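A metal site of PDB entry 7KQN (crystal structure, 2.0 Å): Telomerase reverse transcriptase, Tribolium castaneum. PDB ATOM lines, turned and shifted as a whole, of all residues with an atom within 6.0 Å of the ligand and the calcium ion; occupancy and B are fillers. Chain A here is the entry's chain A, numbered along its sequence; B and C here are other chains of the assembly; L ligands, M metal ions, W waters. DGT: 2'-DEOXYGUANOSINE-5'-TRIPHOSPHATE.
The side-chain amino group (NZ) of Lys 189 is in salt-bridge range of an oxygen (O1G) of the ligand, at 2.9 Å. ND2 of Asn 369 sits close to O2G of the ligand (3.4 Å). A nitrogen (N2) of the ligand is in hydrogen-bond range of O2 of C 10 of chain B, at 2.7 Å. An oxygen (O2B) of the ligand lies close to the backbone NH of Ala 255 (3.0 Å). An oxygen (O1A) of the ligand is in salt-bridge range of the guanidinium group (NH2) of Arg 194, 2.9 Å away. N3 of C 11 of chain B is in hydrogen-bond range of N1 of the ligand, 3.4 Å away. N of Tyr 256 is in hydrogen-bond range of O3' of the ligand. The backbone NH of Asp 254 is in hydrogen-bond range of an oxygen (O3G) of the ligand (3.1 Å). The side-chain amino group (NZ) of Lys 372 lies close to an oxygen (O2G) of the ligand.
O3' of DG 7 of chain C sits close to the side-chain carboxylate of Asp 343, at 2.7 Å. N of Gly 257 lies within hydrogen-bond range of OD1 of Asp 254, 3.5 Å away. The guanidinium group of Arg 194 is in hydrogen-bond range of the side-chain amide oxygen of Gln 308, 3.1 Å away. O of Asp 251 sits at hydrogen-bond distance from N of Asn 369, at 2.8 Å. The side-chain amino group of Lys 372 lies close to the side-chain carboxylate of Asp 251 (3.6 Å). The backbone carbonyl oxygen of Lys 189 lies close to the side-chain amide oxygen of Asn 192.
N2 of the ligand sits close to N of Gly 309, at 3.1 Å. O3' of DG 7 of chain C lies close to an oxygen (O2A) of the ligand. Residues that only touch the ligand: Gln 308 and Arg 253. Hydrophobic or aromatic side chains within 4 Å of the ligand: Ala 255 and Tyr 256. 16 residues have an atom within 4 Å of the ligand: Lys 189, Arg 194, Asp 251, Ile 252, Arg 253, Asp 254, Ala 255, Tyr 256, Gln 308, Gly 309, Asp 343, Asn 369, Lys 372, C 10 of chain B, C 11 of chain B and DG 7 of chain C. Along chain A the residues within 4 Å of the ligand span positions 189 to 372.
Residues that only touch the calcium ion: Lys 372 (3.8 Å). Of the 23 residues printed, 4 come within 4 Å of the calcium ion.
The calcium ion is bound by O of Ile 252 (2.3 Å), OD2 of Asp 343 (2.3 Å), OD1 of Asp 251 (2.3 Å), O2B of the ligand (2.3 Å), O2A of the ligand (2.4 Å), O2G of the ligand (2.4 Å) and OD2 of Asp 251 (2.8 Å).
Water W3 lies within hydrogen-bond range of an oxygen (O3G) of the ligand (2.8 Å) and the guanidinium group (NE) of Arg 253 (2.9 Å). Water W1 bridges NZ of Lys 372 and O3' of DG 7 of chain C.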
ATOM      1  N   LEU A 141      17.397  -0.037  25.310  1.00  0.00           N
ATOM      2  CA  LEU A 141      18.733  -0.283  25.846  1.00  0.00           C
ATOM      3  C   LEU A 141      19.644   0.914  25.558  1.00  0.00           C
ATOM      4  O   LEU A 141      20.870   0.829  25.788  1.00  0.00           O
ATOM      5  CB  LEU A 141      19.369  -1.560  25.283  1.00  0.00           C
ATOM      6  CG  LEU A 141      18.894  -2.901  25.854  1.00  0.00           C
ATOM      7  CD1 LEU A 141      19.116  -3.063  27.353  1.00  0.00           C
ATOM      8  CD2 LEU A 141      17.452  -3.201  25.485  1.00  0.00           C
ATOM      9  N   LYS A 189      17.637  -4.898  18.298  1.00  0.00           N
ATOM     10  CA  LYS A 189      18.973  -4.250  18.456  1.00  0.00           C
ATOM     11  C   LYS A 189      19.391  -3.535  17.169  1.00  0.00           C
ATOM     12  O   LYS A 189      20.197  -4.129  16.424  1.00  0.00           O
ATOM     13  CB  LYS A 189      20.024  -5.291  18.847  1.00  0.00           C
ATOM     14  CG  LYS A 189      20.784  -5.013  20.130  1.00  0.00           C
ATOM     15  CD  LYS A 189      22.244  -4.711  19.902  1.00  0.00           C
ATOM     16  CE  LYS A 189      22.764  -5.261  18.597  1.00  0.00           C
ATOM     17  NZ  LYS A 189      23.967  -6.112  18.808  1.00  0.00           N
ATOM     18  N   ASN A 192      18.883  -5.406  14.198  1.00  0.00           N
ATOM     19  CA  ASN A 192      19.311  -6.792  14.505  1.00  0.00           C
ATOM     20  C   ASN A 192      18.582  -7.187  15.793  1.00  0.00           C
ATOM     21  O   ASN A 192      17.592  -6.518  16.136  1.00  0.00           O
ATOM     22  CB  ASN A 192      20.828  -6.912  14.639  1.00  0.00           C
ATOM     23  CG  ASN A 192      21.591  -5.987  13.707  1.00  0.00           C
ATOM     24  OD1 ASN A 192      22.142  -4.980  14.144  1.00  0.00           O
ATOM     25  ND2 ASN A 192      21.612  -6.321  12.433  1.00  0.00           N
ATOM     26  N   ARG A 194      18.966  -9.235  19.968  1.00  0.00           N
ATOM     27  CA  ARG A 194      19.841  -9.815  21.011  1.00  0.00           C
ATOM     28  C   ARG A 194      19.036 -10.909  21.720  1.00  0.00           C
ATOM     29  O   ARG A 194      18.088 -10.551  22.444  1.00  0.00           O
ATOM     30  CB  ARG A 194      20.361  -8.779  22.007  1.00  0.00           C
ATOM     31  CG  ARG A 194      21.380  -9.341  22.982  1.00  0.00           C
ATOM     32  CD  ARG A 194      21.935  -8.337  23.966  1.00  0.00           C
ATOM     33  NE  ARG A 194      22.650  -7.253  23.332  1.00  0.00           N
ATOM     34  CZ  ARG A 194      23.905  -7.324  22.912  1.00  0.00           C
ATOM     35  NH1 ARG A 194      24.609  -8.437  23.056  1.00  0.00           N
ATOM     36  NH2 ARG A 194      24.466  -6.266  22.341  1.00  0.00           N
ATOM     37  N   ILE A 196      18.555 -13.274  24.568  1.00  0.00           N
ATOM     38  CA  ILE A 196      19.046 -13.417  25.930  1.00  0.00           C
ATOM     39  C   ILE A 196      18.162 -14.417  26.646  1.00  0.00           C
ATOM     40  O   ILE A 196      17.019 -14.663  26.242  1.00  0.00           O
ATOM     41  CB  ILE A 196      19.038 -12.081  26.715  1.00  0.00           C
ATOM     42  CG1 ILE A 196      17.591 -11.625  26.970  1.00  0.00           C
ATOM     43  CG2 ILE A 196      19.827 -10.994  25.993  1.00  0.00           C
ATOM     44  CD1 ILE A 196      17.471 -10.690  28.091  1.00  0.00           C
ATOM     45  N   ASP A 251      35.542  -5.663  16.330  1.00  0.00           N
ATOM     46  CA  ASP A 251      34.542  -6.262  17.205  1.00  0.00           C
ATOM     47  C   ASP A 251      34.206  -7.655  16.697  1.00  0.00           C
ATOM     48  O   ASP A 251      34.012  -7.832  15.490  1.00  0.00           O
ATOM     49  CB  ASP A 251      33.255  -5.425  17.246  1.00  0.00           C
ATOM     50  CG  ASP A 251      32.170  -6.100  18.081  1.00  0.00           C
ATOM     51  OD1 ASP A 251      31.324  -6.810  17.471  1.00  0.00           O
ATOM     52  OD2 ASP A 251      32.079  -5.839  19.286  1.00  0.00           O
ATOM     53  N   ILE A 252      34.120  -8.646  17.586  1.00  0.00           N
ATOM     54  CA  ILE A 252      33.735  -9.996  17.160  1.00  0.00           C
ATOM     55  C   ILE A 252      32.233 -10.045  16.943  1.00  0.00           C
ATOM     56  O   ILE A 252      31.458  -9.555  17.770  1.00  0.00           O
ATOM     57  CB  ILE A 252      34.188 -11.051  18.171  1.00  0.00           C
ATOM     58  CG1 ILE A 252      35.709 -11.040  18.277  1.00  0.00           C
ATOM     59  CG2 ILE A 252      33.696 -12.476  17.755  1.00  0.00           C
ATOM     60  CD1 ILE A 252      36.229 -11.888  19.436  1.00  0.00           C
ATOM     61  N   ARG A 253      31.811 -10.650  15.843  1.00  0.00           N
ATOM     62  CA  ARG A 253      30.391 -10.835  15.624  1.00  0.00           C
ATOM     63  C   ARG A 253      29.818 -11.899  16.588  1.00  0.00           C
ATOM     64  O   ARG A 253      30.399 -12.980  16.731  1.00  0.00           O
ATOM     65  CB  ARG A 253      30.148 -11.234  14.178  1.00  0.00           C
ATOM     66  CG  ARG A 253      28.750 -11.673  13.872  1.00  0.00           C
ATOM     67  CD  ARG A 253      28.601 -11.964  12.405  1.00  0.00           C
ATOM     68  NE  ARG A 253      28.320 -10.723  11.691  1.00  0.00           N
ATOM     69  CZ  ARG A 253      28.648 -10.492  10.422  1.00  0.00           C
ATOM     70  NH1 ARG A 253      29.259 -11.445   9.719  1.00  0.00           N
ATOM     71  NH2 ARG A 253      28.361  -9.326   9.858  1.00  0.00           N
ATOM     72  N   ASP A 254      28.696 -11.597  17.250  1.00  0.00           N
ATOM     73  CA  ASP A 254      27.969 -12.610  18.034  1.00  0.00           C
ATOM     74  C   ASP A 254      28.917 -13.332  18.985  1.00  0.00           C
ATOM     75  O   ASP A 254      29.075 -14.554  18.932  1.00  0.00           O
ATOM     76  CB  ASP A 254      27.309 -13.624  17.082  1.00  0.00           C
ATOM     77  CG  ASP A 254      26.230 -14.506  17.753  1.00  0.00           C
ATOM     78  OD1 ASP A 254      26.000 -14.413  18.986  1.00  0.00           O
ATOM     79  OD2 ASP A 254      25.588 -15.276  16.988  1.00  0.00           O
ATOM     80  N   ALA A 255      29.577 -12.547  19.833  1.00  0.00           N
ATOM     81  CA  ALA A 255      30.745 -13.072  20.552  1.00  0.00           C
ATOM     82  C   ALA A 255      30.404 -14.315  21.387  1.00  0.00           C
ATOM     83  O   ALA A 255      31.056 -15.353  21.239  1.00  0.00           O
ATOM     84  CB  ALA A 255      31.335 -11.994  21.442  1.00  0.00           C
ATOM     85  N   TYR A 256      29.398 -14.236  22.269  1.00  0.00           N
ATOM     86  CA  TYR A 256      29.078 -15.400  23.110  1.00  0.00           C
ATOM     87  C   TYR A 256      28.631 -16.573  22.261  1.00  0.00           C
ATOM     88  O   TYR A 256      28.950 -17.733  22.582  1.00  0.00           O
ATOM     89  CB  TYR A 256      27.965 -15.083  24.118  1.00  0.00           C
ATOM     90  CG  TYR A 256      28.363 -14.340  25.376  1.00  0.00           C
ATOM     91  CD1 TYR A 256      29.530 -13.559  25.409  1.00  0.00           C
ATOM     92  CD2 TYR A 256      27.548 -14.367  26.506  1.00  0.00           C
ATOM     93  CE1 TYR A 256      29.878 -12.847  26.557  1.00  0.00           C
ATOM     94  CE2 TYR A 256      27.888 -13.685  27.643  1.00  0.00           C
ATOM     95  CZ  TYR A 256      29.045 -12.912  27.671  1.00  0.00           C
ATOM     96  OH  TYR A 256      29.355 -12.231  28.823  1.00  0.00           O
ATOM     97  N   GLY A 257      27.866 -16.305  21.205  1.00  0.00           N
ATOM     98  CA  GLY A 257      27.352 -17.345  20.359  1.00  0.00           C
ATOM     99  C   GLY A 257      28.427 -18.111  19.632  1.00  0.00           C
ATOM    100  O   GLY A 257      28.214 -19.279  19.276  1.00  0.00           O
ATOM    101  N   GLN A 308      23.598 -15.798  26.461  1.00  0.00           N
ATOM    102  CA  GLN A 308      23.714 -14.438  26.999  1.00  0.00           C
ATOM    103  C   GLN A 308      22.618 -14.194  28.036  1.00  0.00           C
ATOM    104  O   GLN A 308      21.437 -14.306  27.733  1.00  0.00           O
ATOM    105  CB  GLN A 308      23.581 -13.393  25.896  1.00  0.00           C
ATOM    106  CG  GLN A 308      24.619 -13.494  24.795  1.00  0.00           C
ATOM    107  CD  GLN A 308      24.269 -12.553  23.652  1.00  0.00           C
ATOM    108  OE1 GLN A 308      24.164 -11.349  23.862  1.00  0.00           O
ATOM    109  NE2 GLN A 308      24.037 -13.102  22.470  1.00  0.00           N
ATOM    110  N   GLY A 309      23.035 -13.806  29.238  1.00  0.00           N
ATOM    111  CA  GLY A 309      22.125 -13.632  30.364  1.00  0.00           C
ATOM    112  C   GLY A 309      22.275 -14.697  31.418  1.00  0.00           C
ATOM    113  O   GLY A 309      21.614 -14.608  32.455  1.00  0.00           O
ATOM    114  N   ASP A 310      23.070 -15.722  31.159  1.00  0.00           N
ATOM    115  CA  ASP A 310      23.381 -16.672  32.226  1.00  0.00           C
ATOM    116  C   ASP A 310      24.544 -16.115  33.037  1.00  0.00           C
ATOM    117  O   ASP A 310      25.519 -15.633  32.453  1.00  0.00           O
ATOM    118  CB  ASP A 310      23.757 -18.047  31.665  1.00  0.00           C
ATOM    119  CG  ASP A 310      24.146 -19.036  32.748  1.00  0.00           C
ATOM    120  OD1 ASP A 310      23.228 -19.636  33.344  1.00  0.00           O
ATOM    121  OD2 ASP A 310      25.355 -19.158  33.075  1.00  0.00           O
ATOM    122  N   VAL A 342      36.387  -7.605  26.478  1.00  0.00           N
ATOM    123  CA  VAL A 342      35.451  -8.687  26.058  1.00  0.00           C
ATOM    124  C   VAL A 342      35.809  -9.105  24.622  1.00  0.00           C
ATOM    125  O   VAL A 342      36.847  -9.756  24.461  1.00  0.00           O
ATOM    126  CB  VAL A 342      33.967  -8.350  26.277  1.00  0.00           C
ATOM    127  CG1 VAL A 342      33.064  -9.552  26.061  1.00  0.00           C
ATOM    128  CG2 VAL A 342      33.733  -7.762  27.657  1.00  0.00           C
ATOM    129  N   ASP A 343      34.971  -8.777  23.647  1.00  0.00           N
ATOM    130  CA  ASP A 343      35.192  -9.189  22.234  1.00  0.00           C
ATOM    131  C   ASP A 343      35.737  -8.032  21.382  1.00  0.00           C
ATOM    132  O   ASP A 343      35.744  -8.170  20.152  1.00  0.00           O
ATOM    133  CB  ASP A 343      33.894  -9.699  21.620  1.00  0.00           C
ATOM    134  CG  ASP A 343      32.779  -8.674  21.601  1.00  0.00           C
ATOM    135  OD1 ASP A 343      32.633  -7.953  22.603  1.00  0.00           O
ATOM    136  OD2 ASP A 343      32.056  -8.608  20.587  1.00  0.00           O
ATOM    137  N   ASP A 344      36.141  -6.914  22.009  1.00  0.00           N
ATOM    138  CA  ASP A 344      36.596  -5.738  21.221  1.00  0.00           C
ATOM    139  C   ASP A 344      38.104  -5.555  21.339  1.00  0.00           C
ATOM    140  O   ASP A 344      38.598  -5.517  22.468  1.00  0.00           O
ATOM    141  CB  ASP A 344      35.851  -4.461  21.623  1.00  0.00           C
ATOM    142  CG  ASP A 344      34.412  -4.471  21.152  1.00  0.00           C
ATOM    143  OD1 ASP A 344      34.095  -5.314  20.309  1.00  0.00           O
ATOM    144  OD2 ASP A 344      33.633  -3.634  21.636  1.00  0.00           O
ATOM    145  N   ASN A 369      32.698  -8.407  13.127  1.00  0.00           N
ATOM    146  CA  ASN A 369      31.558  -7.567  12.780  1.00  0.00           C
ATOM    147  C   ASN A 369      32.095  -6.382  11.982  1.00  0.00           C
ATOM    148  O   ASN A 369      32.623  -5.435  12.575  1.00  0.00           O
ATOM    149  CB  ASN A 369      30.832  -7.105  14.035  1.00  0.00           C
ATOM    150  CG  ASN A 369      29.582  -6.324  13.747  1.00  0.00           C
ATOM    151  OD1 ASN A 369      29.254  -6.033  12.600  1.00  0.00           O
ATOM    152  ND2 ASN A 369      28.857  -5.977  14.800  1.00  0.00           N
ATOM    153  N   LYS A 372      31.358  -2.508  12.773  1.00  0.00           N
ATOM    154  CA  LYS A 372      31.950  -1.867  13.936  1.00  0.00           C
ATOM    155  C   LYS A 372      33.430  -1.544  13.762  1.00  0.00           C
ATOM    156  O   LYS A 372      34.029  -0.935  14.659  1.00  0.00           O
ATOM    157  CB  LYS A 372      31.763  -2.763  15.165  1.00  0.00           C
ATOM    158  CG  LYS A 372      30.295  -2.924  15.621  1.00  0.00           C
ATOM    159  CD  LYS A 372      30.218  -3.505  17.042  1.00  0.00           C
ATOM    160  CE  LYS A 372      28.863  -4.160  17.326  1.00  0.00           C
ATOM    161  NZ  LYS A 372      28.755  -4.692  18.743  1.00  0.00           N
ATOM    162  P     C B  10      15.867  -7.311  33.533  1.00  0.00           P
ATOM    163  OP1   C B  10      14.679  -7.316  34.357  1.00  0.00           O
ATOM    164  OP2   C B  10      16.717  -6.092  33.492  1.00  0.00           O
ATOM    165  O5'   C B  10      16.858  -8.499  33.948  1.00  0.00           O
ATOM    166  C5'   C B  10      16.392  -9.845  34.029  1.00  0.00           C
ATOM    167  C4'   C B  10      17.412 -10.822  33.511  1.00  0.00           C
ATOM    168  O4'   C B  10      17.471 -10.759  32.059  1.00  0.00           O
ATOM    169  C3'   C B  10      18.856 -10.569  33.928  1.00  0.00           C
ATOM    170  O3'   C B  10      19.136 -11.016  35.242  1.00  0.00           O
ATOM    171  C2'   C B  10      19.630 -11.296  32.842  1.00  0.00           C
ATOM    172  O2'   C B  10      19.588 -12.719  33.028  1.00  0.00           O
ATOM    173  C1'   C B  10      18.789 -10.953  31.616  1.00  0.00           C
ATOM    174  N1    C B  10      19.232  -9.707  30.963  1.00  0.00           N
ATOM    175  C2    C B  10      20.384  -9.728  30.185  1.00  0.00           C
ATOM    176  O2    C B  10      21.013 -10.800  30.056  1.00  0.00           O
ATOM    177  N3    C B  10      20.805  -8.596  29.581  1.00  0.00           N
ATOM    178  C4    C B  10      20.102  -7.471  29.734  1.00  0.00           C
ATOM    179  N4    C B  10      20.559  -6.368  29.132  1.00  0.00           N
ATOM    180  C5    C B  10      18.912  -7.426  30.539  1.00  0.00           C
ATOM    181  C6    C B  10      18.524  -8.548  31.128  1.00  0.00           C
ATOM    182  P     C B  11      20.265 -10.309  36.109  1.00  0.00           P
ATOM    183  OP1   C B  11      20.253 -10.893  37.465  1.00  0.00           O
ATOM    184  OP2   C B  11      20.253  -8.836  35.869  1.00  0.00           O
ATOM    185  O5'   C B  11      21.625 -10.740  35.405  1.00  0.00           O
ATOM    186  C5'   C B  11      21.943 -12.108  35.158  1.00  0.00           C
ATOM    187  C4'   C B  11      23.254 -12.220  34.407  1.00  0.00           C
ATOM    188  O4'   C B  11      23.117 -11.646  33.070  1.00  0.00           O
ATOM    189  C3'   C B  11      24.412 -11.436  35.003  1.00  0.00           C
ATOM    190  O3'   C B  11      24.985 -12.107  36.106  1.00  0.00           O
ATOM    191  C2'   C B  11      25.348 -11.283  33.799  1.00  0.00           C
ATOM    192  O2'   C B  11      26.019 -12.506  33.521  1.00  0.00           O
ATOM    193  C1'   C B  11      24.339 -11.084  32.663  1.00  0.00           C
ATOM    194  N1    C B  11      24.146  -9.666  32.256  1.00  0.00           N
ATOM    195  C2    C B  11      25.156  -9.079  31.481  1.00  0.00           C
ATOM    196  O2    C B  11      26.163  -9.736  31.193  1.00  0.00           O
ATOM    197  N3    C B  11      25.028  -7.806  31.045  1.00  0.00           N
ATOM    198  C4    C B  11      23.947  -7.097  31.343  1.00  0.00           C
ATOM    199  N4    C B  11      23.921  -5.852  30.886  1.00  0.00           N
ATOM    200  C5    C B  11      22.885  -7.657  32.144  1.00  0.00           C
ATOM    201  C6    C B  11      23.012  -8.932  32.567  1.00  0.00           C
ATOM    202  P    DG C   7      31.900  -0.720  24.364  1.00  0.00           P
ATOM    203  OP1  DG C   7      32.771  -0.480  23.224  1.00  0.00           O
ATOM    204  OP2  DG C   7      30.520  -0.208  24.434  1.00  0.00           O
ATOM    205  O5'  DG C   7      31.728  -2.336  24.566  1.00  0.00           O
ATOM    206  C5'  DG C   7      32.842  -3.198  24.368  1.00  0.00           C
ATOM    207  C4'  DG C   7      32.445  -4.612  24.739  1.00  0.00           C
ATOM    208  O4'  DG C   7      32.061  -4.660  26.132  1.00  0.00           O
ATOM    209  C3'  DG C   7      31.230  -5.113  24.029  1.00  0.00           C
ATOM    210  O3'  DG C   7      31.583  -5.520  22.684  1.00  0.00           O
ATOM    211  C2'  DG C   7      30.831  -6.270  24.935  1.00  0.00           C
ATOM    212  C1'  DG C   7      31.095  -5.677  26.317  1.00  0.00           C
ATOM    213  N9   DG C   7      29.856  -5.120  26.934  1.00  0.00           N
ATOM    214  C8   DG C   7      29.310  -3.875  26.766  1.00  0.00           C
ATOM    215  N7   DG C   7      28.175  -3.736  27.417  1.00  0.00           N
ATOM    216  C5   DG C   7      27.956  -4.960  28.049  1.00  0.00           C
ATOM    217  C6   DG C   7      26.873  -5.406  28.888  1.00  0.00           C
ATOM    218  O6   DG C   7      25.871  -4.782  29.265  1.00  0.00           O
ATOM    219  N1   DG C   7      27.053  -6.705  29.312  1.00  0.00           N
ATOM    220  C2   DG C   7      28.101  -7.515  28.961  1.00  0.00           C
ATOM    221  N2   DG C   7      28.098  -8.758  29.461  1.00  0.00           N
ATOM    222  N3   DG C   7      29.113  -7.118  28.171  1.00  0.00           N
ATOM    223  C4   DG C   7      28.977  -5.817  27.774  1.00  0.00           C
HETATM  224  PG  DGT L   1      27.219  -8.248  17.281  1.00  0.00           P
HETATM  225  O1G DGT L   1      26.018  -7.331  17.204  1.00  0.00           O
HETATM  226  O2G DGT L   1      28.476  -7.562  17.792  1.00  0.00           O
HETATM  227  O3G DGT L   1      27.466  -9.035  16.013  1.00  0.00           O
HETATM  228  O3B DGT L   1      26.672  -9.352  18.511  1.00  0.00           O
HETATM  229  PB  DGT L   1      27.357  -9.614  19.903  1.00  0.00           P
HETATM  230  O1B DGT L   1      26.607 -10.690  20.630  1.00  0.00           O
HETATM  231  O2B DGT L   1      28.841  -9.637  19.900  1.00  0.00           O
HETATM  232  O3A DGT L   1      27.029  -8.322  21.041  1.00  0.00           O
HETATM  233  PA  DGT L   1      27.986  -7.213  21.571  1.00  0.00           P
HETATM  234  O1A DGT L   1      27.309  -6.068  22.255  1.00  0.00           O
HETATM  235  O2A DGT L   1      29.266  -6.940  20.852  1.00  0.00           O
HETATM  236  O5' DGT L   1      28.808  -7.876  23.051  1.00  0.00           O
HETATM  237  C5' DGT L   1      29.594  -8.933  22.952  1.00  0.00           C
HETATM  238  C4' DGT L   1      29.155  -9.990  24.012  1.00  0.00           C
HETATM  239  O4' DGT L   1      28.920  -9.322  25.263  1.00  0.00           O
HETATM  240  C3' DGT L   1      27.799 -10.574  23.628  1.00  0.00           C
HETATM  241  O3' DGT L   1      27.936 -11.725  22.842  1.00  0.00           O
HETATM  242  C2' DGT L   1      27.290 -10.937  24.972  1.00  0.00           C
HETATM  243  C1' DGT L   1      27.844  -9.853  25.926  1.00  0.00           C
HETATM  244  N9  DGT L   1      26.810  -8.823  26.140  1.00  0.00           N
HETATM  245  C8  DGT L   1      26.808  -7.547  25.551  1.00  0.00           C
HETATM  246  N7  DGT L   1      25.735  -6.833  25.913  1.00  0.00           N
HETATM  247  C5  DGT L   1      24.981  -7.667  26.750  1.00  0.00           C
HETATM  248  C6  DGT L   1      23.777  -7.566  27.464  1.00  0.00           C
HETATM  249  O6  DGT L   1      23.052  -6.418  27.402  1.00  0.00           O
HETATM  250  N1  DGT L   1      23.287  -8.571  28.213  1.00  0.00           N
HETATM  251  C2  DGT L   1      24.036  -9.737  28.262  1.00  0.00           C
HETATM  252  N2  DGT L   1      23.540 -10.790  29.038  1.00  0.00           N
HETATM  253  N3  DGT L   1      25.218  -9.979  27.635  1.00  0.00           N
HETATM  254  C4  DGT L   1      25.655  -8.928  26.889  1.00  0.00           C
HETATM  255 CA    CA M   1      30.412  -8.073  19.124  1.00  0.00          CA
HETATM  256  O   HOH W   1      30.266  -4.129  20.712  1.00  0.00           O
HETATM  257  O   HOH W   2      25.074 -10.684  15.963  1.00  0.00           O
HETATM  258  O   HOH W   3      26.673  -8.958  13.342  1.00  0.00           O
HETATM  259  O   HOH W   4      26.194  -4.489  20.109  1.00  0.00           O
HETATM  260  O   HOH W   5      25.383  -4.172  25.279  1.00  0.00           O
HETATM  261  O   HOH W   6      27.728  -4.252  23.961  1.00  0.00           O
